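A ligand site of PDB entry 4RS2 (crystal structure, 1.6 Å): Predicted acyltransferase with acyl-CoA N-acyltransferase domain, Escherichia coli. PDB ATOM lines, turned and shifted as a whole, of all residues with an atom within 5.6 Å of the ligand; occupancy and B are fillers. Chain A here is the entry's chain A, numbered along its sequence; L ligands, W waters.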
ATOM      1  N   SER A  37       2.670  -9.667  -8.170  1.00  0.00           N
ATOM      2  CA  SER A  37       3.531 -10.634  -7.472  1.00  0.00           C
ATOM      3  C   SER A  37       4.899 -10.883  -8.074  1.00  0.00           C
ATOM      4  O   SER A  37       5.816 -11.307  -7.361  1.00  0.00           O
ATOM      5  CB  SER A  37       2.833 -11.977  -7.373  1.00  0.00           C
ATOM      6  OG  SER A  37       1.687 -11.860  -6.547  1.00  0.00           O
ATOM      7  N   PHE A  38       5.052 -10.627  -9.375  1.00  0.00           N
ATOM      8  CA  PHE A  38       6.288 -10.829 -10.060  1.00  0.00           C
ATOM      9  C   PHE A  38       6.936  -9.520 -10.409  1.00  0.00           C
ATOM     10  O   PHE A  38       6.296  -8.473 -10.384  1.00  0.00           O
ATOM     11  CB  PHE A  38       6.088 -11.730 -11.281  1.00  0.00           C
ATOM     12  CG  PHE A  38       5.723 -13.134 -10.897  1.00  0.00           C
ATOM     13  CD1 PHE A  38       6.698 -14.034 -10.595  1.00  0.00           C
ATOM     14  CD2 PHE A  38       4.406 -13.521 -10.782  1.00  0.00           C
ATOM     15  CE1 PHE A  38       6.403 -15.327 -10.212  1.00  0.00           C
ATOM     16  CE2 PHE A  38       4.085 -14.814 -10.366  1.00  0.00           C
ATOM     17  CZ  PHE A  38       5.083 -15.710 -10.084  1.00  0.00           C
ATOM     18  N   GLU A  39       8.219  -9.601 -10.736  1.00  0.00           N
ATOM     19  CA  GLU A  39       9.040  -8.435 -11.069  1.00  0.00           C
ATOM     20  C   GLU A  39       8.698  -7.833 -12.459  1.00  0.00           C
ATOM     21  O   GLU A  39       9.058  -6.705 -12.763  1.00  0.00           O
ATOM     22  CB  GLU A  39      10.534  -8.812 -10.995  1.00  0.00           C
ATOM     23  CG  GLU A  39      11.079  -8.990  -9.562  1.00  0.00           C
ATOM     24  CD  GLU A  39      12.453  -9.680  -9.475  1.00  0.00           C
ATOM     25  OE1 GLU A  39      12.710 -10.677 -10.213  1.00  0.00           O
ATOM     26  OE2 GLU A  39      13.290  -9.275  -8.639  1.00  0.00           O
ATOM     27  N   LEU A  93       3.531 -19.857  -9.941  1.00  0.00           N
ATOM     28  CA  LEU A  93       3.085 -20.126  -8.593  1.00  0.00           C
ATOM     29  C   LEU A  93       3.196 -18.828  -7.841  1.00  0.00           C
ATOM     30  O   LEU A  93       4.276 -18.235  -7.758  1.00  0.00           O
ATOM     31  CB  LEU A  93       3.970 -21.185  -7.927  1.00  0.00           C
ATOM     32  CG  LEU A  93       3.704 -21.425  -6.435  1.00  0.00           C
ATOM     33  CD1 LEU A  93       2.307 -21.963  -6.262  1.00  0.00           C
ATOM     34  CD2 LEU A  93       4.743 -22.382  -5.847  1.00  0.00           C
ATOM     35  N   ALA A  94       2.089 -18.372  -7.285  1.00  0.00           N
ATOM     36  CA  ALA A  94       2.069 -17.090  -6.602  1.00  0.00           C
ATOM     37  C   ALA A  94       1.107 -17.040  -5.446  1.00  0.00           C
ATOM     38  O   ALA A  94       0.016 -17.576  -5.536  1.00  0.00           O
ATOM     39  CB  ALA A  94       1.748 -15.987  -7.589  1.00  0.00           C
ATOM     40  N   VAL A  95       1.560 -16.394  -4.380  1.00  0.00           N
ATOM     41  CA  VAL A  95       0.676 -16.101  -3.260  1.00  0.00           C
ATOM     42  C   VAL A  95       0.789 -14.602  -2.967  1.00  0.00           C
ATOM     43  O   VAL A  95       1.890 -14.025  -2.936  1.00  0.00           O
ATOM     44  CB  VAL A  95       1.050 -16.936  -2.034  1.00  0.00           C
ATOM     45  CG1 VAL A  95       0.290 -16.475  -0.808  1.00  0.00           C
ATOM     46  CG2 VAL A  95       0.818 -18.413  -2.322  1.00  0.00           C
ATOM     47  N   ASP A  96      -0.384 -13.965  -2.794  1.00  0.00           N
ATOM     48  CA  ASP A  96      -0.444 -12.525  -2.503  1.00  0.00           C
ATOM     49  C   ASP A  96       0.398 -12.226  -1.262  1.00  0.00           C
ATOM     50  O   ASP A  96       0.329 -12.940  -0.297  1.00  0.00           O
ATOM     51  CB  ASP A  96      -1.886 -12.107  -2.289  1.00  0.00           C
ATOM     52  CG  ASP A  96      -2.048 -10.600  -2.181  1.00  0.00           C
ATOM     53  OD1 ASP A  96      -1.401  -9.950  -1.326  1.00  0.00           O
ATOM     54  OD2 ASP A  96      -2.892 -10.020  -2.917  1.00  0.00           O
ATOM     55  N   TYR A  99      -0.789 -12.771   2.281  1.00  0.00           N
ATOM     56  CA  TYR A  99      -1.047 -14.107   2.756  1.00  0.00           C
ATOM     57  C   TYR A  99       0.177 -14.997   2.742  1.00  0.00           C
ATOM     58  O   TYR A  99       0.055 -16.198   2.933  1.00  0.00           O
ATOM     59  CB  TYR A  99      -2.166 -14.740   1.923  1.00  0.00           C
ATOM     60  CG  TYR A  99      -3.504 -14.107   2.176  1.00  0.00           C
ATOM     61  CD1 TYR A  99      -3.909 -12.967   1.503  1.00  0.00           C
ATOM     62  CD2 TYR A  99      -4.368 -14.654   3.110  1.00  0.00           C
ATOM     63  CE1 TYR A  99      -5.125 -12.381   1.761  1.00  0.00           C
ATOM     64  CE2 TYR A  99      -5.601 -14.085   3.370  1.00  0.00           C
ATOM     65  CZ  TYR A  99      -5.965 -12.945   2.698  1.00  0.00           C
ATOM     66  OH  TYR A  99      -7.198 -12.381   2.968  1.00  0.00           O
ATOM     67  N   ARG A 100       1.365 -14.418   2.602  1.00  0.00           N
ATOM     68  CA  ARG A 100       2.558 -15.259   2.587  1.00  0.00           C
ATOM     69  C   ARG A 100       2.914 -15.805   3.938  1.00  0.00           C
ATOM     70  O   ARG A 100       2.607 -15.212   4.980  1.00  0.00           O
ATOM     71  CB  ARG A 100       3.741 -14.565   1.947  1.00  0.00           C
ATOM     72  CG  ARG A 100       3.559 -14.455   0.464  1.00  0.00           C
ATOM     73  CD  ARG A 100       4.668 -13.690  -0.201  1.00  0.00           C
ATOM     74  NE  ARG A 100       4.226 -13.377  -1.544  1.00  0.00           N
ATOM     75  CZ  ARG A 100       4.793 -12.497  -2.344  1.00  0.00           C
ATOM     76  NH1 ARG A 100       5.874 -11.835  -1.941  1.00  0.00           N
ATOM     77  NH2 ARG A 100       4.284 -12.260  -3.538  1.00  0.00           N
ATOM     78  N   GLY A 101       3.557 -16.986   3.883  1.00  0.00           N
ATOM     79  CA  GLY A 101       4.002 -17.731   5.055  1.00  0.00           C
ATOM     80  C   GLY A 101       2.888 -18.471   5.787  1.00  0.00           C
ATOM     81  O   GLY A 101       3.086 -18.908   6.928  1.00  0.00           O
ATOM     82  N   GLN A 102       1.735 -18.632   5.141  1.00  0.00           N
ATOM     83  CA  GLN A 102       0.588 -19.320   5.741  1.00  0.00           C
ATOM     84  C   GLN A 102       0.429 -20.759   5.242  1.00  0.00           C
ATOM     85  O   GLN A 102      -0.530 -21.450   5.616  1.00  0.00           O
ATOM     86  CB  GLN A 102      -0.708 -18.540   5.479  1.00  0.00           C
ATOM     87  CG  GLN A 102      -0.771 -17.186   6.128  1.00  0.00           C
ATOM     88  CD  GLN A 102      -2.094 -16.464   5.926  1.00  0.00           C
ATOM     89  OE1 GLN A 102      -3.096 -17.054   5.515  1.00  0.00           O
ATOM     90  NE2 GLN A 102      -2.085 -15.158   6.156  1.00  0.00           N
ATOM     91  N   GLY A 103       1.349 -21.195   4.378  1.00  0.00           N
ATOM     92  CA  GLY A 103       1.300 -22.535   3.830  1.00  0.00           C
ATOM     93  C   GLY A 103       0.452 -22.687   2.560  1.00  0.00           C
ATOM     94  O   GLY A 103       0.206 -23.799   2.112  1.00  0.00           O
ATOM     95  N   LEU A 104      -0.011 -21.582   1.978  1.00  0.00           N
ATOM     96  CA  LEU A 104      -0.864 -21.630   0.801  1.00  0.00           C
ATOM     97  C   LEU A 104      -0.142 -22.132  -0.457  1.00  0.00           C
ATOM     98  O   LEU A 104      -0.747 -22.809  -1.279  1.00  0.00           O
ATOM     99  CB  LEU A 104      -1.489 -20.254   0.517  1.00  0.00           C
ATOM    100  CG  LEU A 104      -2.647 -19.800   1.369  1.00  0.00           C
ATOM    101  CD1 LEU A 104      -2.979 -18.373   0.978  1.00  0.00           C
ATOM    102  CD2 LEU A 104      -3.843 -20.725   1.146  1.00  0.00           C
ATOM    103  N   ALA A 105       1.135 -21.806  -0.636  1.00  0.00           N
ATOM    104  CA  ALA A 105       1.861 -22.331  -1.817  1.00  0.00           C
ATOM    105  C   ALA A 105       2.009 -23.840  -1.683  1.00  0.00           C
ATOM    106  O   ALA A 105       1.752 -24.568  -2.625  1.00  0.00           O
ATOM    107  CB  ALA A 105       3.191 -21.674  -1.992  1.00  0.00           C
ATOM    108  N   ARG A 106       2.421 -24.294  -0.496  1.00  0.00           N
ATOM    109  CA  ARG A 106       2.491 -25.709  -0.243  1.00  0.00           C
ATOM    110  C   ARG A 106       1.193 -26.418  -0.578  1.00  0.00           C
ATOM    111  O   ARG A 106       1.189 -27.452  -1.245  1.00  0.00           O
ATOM    112  CB  ARG A 106       2.856 -25.983   1.214  1.00  0.00           C
ATOM    113  CG  ARG A 106       2.911 -27.456   1.583  1.00  0.00           C
ATOM    114  CD  ARG A 106       3.501 -27.627   2.977  1.00  0.00           C
ATOM    115  NE  ARG A 106       4.948 -27.512   3.016  1.00  0.00           N
ATOM    116  CZ  ARG A 106       5.776 -28.494   2.664  1.00  0.00           C
ATOM    117  NH1 ARG A 106       5.301 -29.657   2.238  1.00  0.00           N
ATOM    118  NH2 ARG A 106       7.074 -28.331   2.730  1.00  0.00           N
ATOM    119  N   GLN A 107       0.078 -25.870  -0.101  1.00  0.00           N
ATOM    120  CA  GLN A 107      -1.237 -26.438  -0.382  1.00  0.00           C
ATOM    121  C   GLN A 107      -1.605 -26.430  -1.855  1.00  0.00           C
ATOM    122  O   GLN A 107      -2.175 -27.392  -2.356  1.00  0.00           O
ATOM    123  CB  GLN A 107      -2.301 -25.720   0.422  1.00  0.00           C
ATOM    124  CG  GLN A 107      -2.159 -25.980   1.910  1.00  0.00           C
ATOM    125  CD  GLN A 107      -2.964 -25.036   2.799  1.00  0.00           C
ATOM    126  OE1 GLN A 107      -3.314 -23.913   2.418  1.00  0.00           O
ATOM    127  NE2 GLN A 107      -3.230 -25.479   4.017  1.00  0.00           N
ATOM    128  N   ASP A 129      13.858 -22.141  -7.914  1.00  0.00           N
ATOM    129  CA  ASP A 129      14.827 -22.349  -6.875  1.00  0.00           C
ATOM    130  C   ASP A 129      14.608 -23.705  -6.208  1.00  0.00           C
ATOM    131  O   ASP A 129      13.539 -23.946  -5.670  1.00  0.00           O
ATOM    132  CB  ASP A 129      14.672 -21.212  -5.835  1.00  0.00           C
ATOM    133  CG  ASP A 129      15.820 -21.148  -4.859  1.00  0.00           C
ATOM    134  OD1 ASP A 129      16.534 -22.175  -4.639  1.00  0.00           O
ATOM    135  OD2 ASP A 129      15.997 -20.045  -4.285  1.00  0.00           O
ATOM    136  N   ALA A 131      15.655 -24.661  -3.450  1.00  0.00           N
ATOM    137  CA  ALA A 131      15.436 -24.450  -2.020  1.00  0.00           C
ATOM    138  C   ALA A 131      13.935 -24.279  -1.748  1.00  0.00           C
ATOM    139  O   ALA A 131      13.469 -24.498  -0.621  1.00  0.00           O
ATOM    140  CB  ALA A 131      16.235 -23.245  -1.538  1.00  0.00           C
ATOM    141  N   LEU A 132      13.169 -23.882  -2.755  1.00  0.00           N
ATOM    142  CA  LEU A 132      11.732 -23.827  -2.613  1.00  0.00           C
ATOM    143  C   LEU A 132      11.128 -25.176  -3.011  1.00  0.00           C
ATOM    144  O   LEU A 132      10.470 -25.840  -2.191  1.00  0.00           O
ATOM    145  CB  LEU A 132      11.164 -22.710  -3.482  1.00  0.00           C
ATOM    146  CG  LEU A 132       9.660 -22.651  -3.662  1.00  0.00           C
ATOM    147  CD1 LEU A 132       9.001 -22.456  -2.314  1.00  0.00           C
ATOM    148  CD2 LEU A 132       9.252 -21.555  -4.611  1.00  0.00           C
ATOM    149  N   ARG A 135      11.102 -28.718  -1.233  1.00  0.00           N
ATOM    150  CA  ARG A 135      10.215 -28.839  -0.055  1.00  0.00           C
ATOM    151  C   ARG A 135       8.960 -29.565  -0.375  1.00  0.00           C
ATOM    152  O   ARG A 135       8.309 -30.115   0.522  1.00  0.00           O
ATOM    153  CB  ARG A 135       9.846 -27.449   0.453  1.00  0.00           C
ATOM    154  CG  ARG A 135      11.019 -26.629   0.913  1.00  0.00           C
ATOM    155  CD  ARG A 135      10.559 -25.229   1.246  1.00  0.00           C
ATOM    156  NE  ARG A 135      11.688 -24.411   1.658  1.00  0.00           N
ATOM    157  CZ  ARG A 135      12.226 -24.408   2.867  1.00  0.00           C
ATOM    158  NH1 ARG A 135      11.745 -25.200   3.800  1.00  0.00           N
ATOM    159  NH2 ARG A 135      13.273 -23.632   3.124  1.00  0.00           N
ATOM    160  N   PHE A 136       8.597 -29.562  -1.662  1.00  0.00           N
ATOM    161  CA  PHE A 136       7.354 -30.154  -2.117  1.00  0.00           C
ATOM    162  C   PHE A 136       7.607 -31.498  -2.819  1.00  0.00           C
ATOM    163  O   PHE A 136       6.731 -32.036  -3.465  1.00  0.00           O
ATOM    164  CB  PHE A 136       6.633 -29.196  -3.056  1.00  0.00           C
ATOM    165  CG  PHE A 136       6.546 -27.775  -2.543  1.00  0.00           C
ATOM    166  CD1 PHE A 136       6.202 -27.494  -1.217  1.00  0.00           C
ATOM    167  CD2 PHE A 136       6.741 -26.710  -3.403  1.00  0.00           C
ATOM    168  CE1 PHE A 136       6.095 -26.194  -0.751  1.00  0.00           C
ATOM    169  CE2 PHE A 136       6.654 -25.402  -2.943  1.00  0.00           C
ATOM    170  CZ  PHE A 136       6.315 -25.146  -1.608  1.00  0.00           C
ATOM    171  N   CYS A 186      10.208 -16.209 -13.976  1.00  0.00           N
ATOM    172  CA  CYS A 186      10.941 -16.661 -12.797  1.00  0.00           C
ATOM    173  C   CYS A 186      11.631 -18.006 -13.083  1.00  0.00           C
ATOM    174  O   CYS A 186      11.080 -18.872 -13.781  1.00  0.00           O
ATOM    175  CB  CYS A 186       9.981 -16.783 -11.611  1.00  0.00           C
ATOM    176  SG  CYS A 186      10.806 -17.066 -10.027  1.00  0.00           S
ATOM    177  N   GLY A 187      12.866 -18.168 -12.597  1.00  0.00           N
ATOM    178  CA  GLY A 187      13.612 -19.407 -12.786  1.00  0.00           C
ATOM    179  C   GLY A 187      14.530 -19.409 -13.999  1.00  0.00           C
ATOM    180  O   GLY A 187      15.413 -20.240 -14.100  1.00  0.00           O
HETATM  181  N1  LIG L   1      12.721 -19.725  -0.930  1.00  0.00           N
HETATM  182  C1  LIG L   1      12.723 -20.903  -0.270  1.00  0.00           C
HETATM  183  N2  LIG L   1      11.659 -21.356   0.412  1.00  0.00           N
HETATM  184  C2  LIG L   1      10.507 -20.621   0.434  1.00  0.00           C
HETATM  185  C3  LIG L   1      10.435 -19.334  -0.256  1.00  0.00           C
HETATM  186  C4  LIG L   1      11.643 -18.908  -0.966  1.00  0.00           C
HETATM  187  N3  LIG L   1      11.612 -17.735  -1.631  1.00  0.00           N
HETATM  188  N4  LIG L   1       9.215 -18.838  -0.051  1.00  0.00           N
HETATM  189  C5  LIG L   1       8.542 -19.732   0.715  1.00  0.00           C
HETATM  190  N5  LIG L   1       9.316 -20.761   1.025  1.00  0.00           N
HETATM  191  C6  LIG L   1       8.943 -21.949   1.798  1.00  0.00           C
HETATM  192  C7  LIG L   1       8.279 -21.669   3.131  1.00  0.00           C
HETATM  193  O1  LIG L   1       9.232 -21.301   4.143  1.00  0.00           O
HETATM  194  C8  LIG L   1       7.593 -22.976   3.380  1.00  0.00           C
HETATM  195  O2  LIG L   1       8.552 -23.947   3.826  1.00  0.00           O
HETATM  196  P1  LIG L   1       8.109 -25.364   4.487  1.00  0.00           P
HETATM  197  O3  LIG L   1       6.622 -25.550   4.259  1.00  0.00           O
HETATM  198  O4  LIG L   1       8.974 -26.403   3.889  1.00  0.00           O
HETATM  199  O5  LIG L   1       8.440 -25.175   5.930  1.00  0.00           O
HETATM  200  C9  LIG L   1       7.126 -23.383   1.984  1.00  0.00           C
HETATM  201  O6  LIG L   1       7.915 -22.632   1.055  1.00  0.00           O
HETATM  202  C10 LIG L   1       5.658 -23.117   1.748  1.00  0.00           C
HETATM  203  O7  LIG L   1       5.348 -21.776   2.126  1.00  0.00           O
HETATM  204  P2  LIG L   1       3.911 -21.087   1.903  1.00  0.00           P
HETATM  205  O8  LIG L   1       3.545 -20.280   3.110  1.00  0.00           O
HETATM  206  O9  LIG L   1       3.000 -22.158   1.358  1.00  0.00           O
HETATM  207  O10 LIG L   1       4.209 -20.070   0.692  1.00  0.00           O
HETATM  208  P3  LIG L   1       4.444 -18.484   0.721  1.00  0.00           P
HETATM  209  O11 LIG L   1       3.262 -17.755   1.182  1.00  0.00           O
HETATM  210  O12 LIG L   1       5.735 -18.145   1.435  1.00  0.00           O
HETATM  211  O13 LIG L   1       4.588 -18.233  -0.870  1.00  0.00           O
HETATM  212  C11 LIG L   1       5.749 -17.865  -2.960  1.00  0.00           C
HETATM  213  C12 LIG L   1       5.776 -18.520  -1.597  1.00  0.00           C
HETATM  214  C13 LIG L   1       7.049 -18.134  -3.707  1.00  0.00           C
HETATM  215  C14 LIG L   1       4.586 -18.490  -3.714  1.00  0.00           C
HETATM  216  C15 LIG L   1       5.530 -16.356  -2.743  1.00  0.00           C
HETATM  217  O14 LIG L   1       6.618 -15.787  -1.962  1.00  0.00           O
HETATM  218  C16 LIG L   1       5.353 -15.554  -3.998  1.00  0.00           C
HETATM  219  O15 LIG L   1       4.259 -15.495  -4.593  1.00  0.00           O
HETATM  220  N6  LIG L   1       6.420 -14.865  -4.402  1.00  0.00           N
HETATM  221  C17 LIG L   1       6.374 -13.976  -5.545  1.00  0.00           C
HETATM  222  C18 LIG L   1       6.578 -14.751  -6.821  1.00  0.00           C
HETATM  223  C19 LIG L   1       7.988 -15.279  -6.867  1.00  0.00           C
HETATM  224  O16 LIG L   1       8.233 -16.447  -6.623  1.00  0.00           O
HETATM  225  N7  LIG L   1       8.931 -14.402  -7.187  1.00  0.00           N
HETATM  226  C20 LIG L   1      10.321 -14.784  -7.386  1.00  0.00           C
HETATM  227  C21 LIG L   1      10.819 -14.234  -8.721  1.00  0.00           C
HETATM  228  S1  LIG L   1      11.878 -15.435  -9.565  1.00  0.00           S
HETATM  229  O   HOH W   1      14.127 -18.045  -4.017  1.00  0.00           O
HETATM  230  O   HOH W   2       7.012 -18.156  -8.092  1.00  0.00           O
HETATM  231  O   HOH W   3       0.986 -18.674   2.289  1.00  0.00           O
HETATM  232  O   HOH W   4       8.972 -13.824  -3.657  1.00  0.00           O
HETATM  233  O   HOH W   5       8.451 -11.127  -7.064  1.00  0.00           O
HETATM  234  O   HOH W   6       4.345 -24.473   4.781  1.00  0.00           O
HETATM  235  O   HOH W   7       6.930 -20.053   5.731  1.00  0.00           O
HETATM  236  O   HOH W   8      14.647 -16.590 -11.244  1.00  0.00           O
HETATM  237  O   HOH W   9      13.592 -12.933  -8.973  1.00  0.00           O
HETATM  238  O   HOH W  10      15.750 -19.578  -1.529  1.00  0.00           O
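An oxygen (O3) of the ligand is in salt-bridge range of the guanidinium group (NE) of Arg 106 (2.9 Å).
The side-chain sulfur (SG) of Cys 186 is bonded to a sulfur (S1) of the ligand, at 2.0 Å.
The backbone NH (N) of Ala 105 sits at hydrogen-bond distance from an oxygen (O9) of the ligand (2.8 Å).
An oxygen (O9) of the ligand sits at hydrogen-bond distance from the backbone NH (N) of Leu 104 (3.1 Å).
NH1 of Arg 135 is in salt-bridge range of O4 of the ligand, at 3.0 Å.
The backbone NH (N) of Arg 106 lies within hydrogen-bond range of an oxygen (O9) of the ligand, 2.9 Å away.
An oxygen (O11) of the ligand lies within hydrogen-bond range of the backbone NH (N) of Gly 101 (2.8 Å).
The backbone NH (N) of Gln 102 lies within hydrogen-bond range of an oxygen (O8) of the ligand, at 3.2 Å.
An oxygen (O15) of the ligand is in hydrogen-bond range of the backbone NH (N) of Val 95, 2.9 Å away.
An oxygen (O8) of the ligand sits at hydrogen-bond distance from the backbone NH (N) of Gly 103 (2.7 Å).
The guanidinium group of Arg 100 lies close to an oxygen (O15) of the ligand (3.4 Å).
The backbone carbonyl oxygen (O) of Val 95 is in hydrogen-bond range of the guanidinium group (NE) of Arg 100, at 2.8 Å.
NE of Arg 135 is in hydrogen-bond range of O of Ala 131 (2.9 Å).
OD1 of Asp 129 lies within hydrogen-bond range of N of Ala 131 (2.9 Å).
NH2 of Arg 106 is in hydrogen-bond range of O of Arg 135, at 3.1 Å.
Ser 37 touches the ligand (O to C17, 3.3 Å).
Phe 38 touches the ligand (CE1 to C18, 3.4 Å).
Ala 94 touches the ligand.
Tyr 99 touches the ligand.
Ala 131 touches the ligand (O to C1, 3.7 Å).
Leu 132 touches the ligand.
CZ of Phe 136 touches C10 of the ligand (3.98 Å).
Water W2 bridges O16 of the ligand (2.6 Å) and O of Leu 93 (2.8 Å).
Water W9 bridges the side-chain carboxylate of Glu 39 and a sulfur (S1) of the ligand.
Water W10 lies within hydrogen-bond range of the side-chain carboxylate (OD2) of Asp 129 (2.8 Å) and a nitrogen (N1) of the ligand (3.1 Å).
Water W5 bridges the backbone carbonyl oxygen of Ser 37 and a nitrogen (N7) of the ligand.
Water W8 lies within hydrogen-bond range of N of Gly 187 (2.7 Å) and S1 of the ligand (3.4 Å).
Water W1 lies within hydrogen-bond range of the side-chain carboxylate of Asp 129 (2.8 Å) and a nitrogen (N3) of the ligand (3.5 Å).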
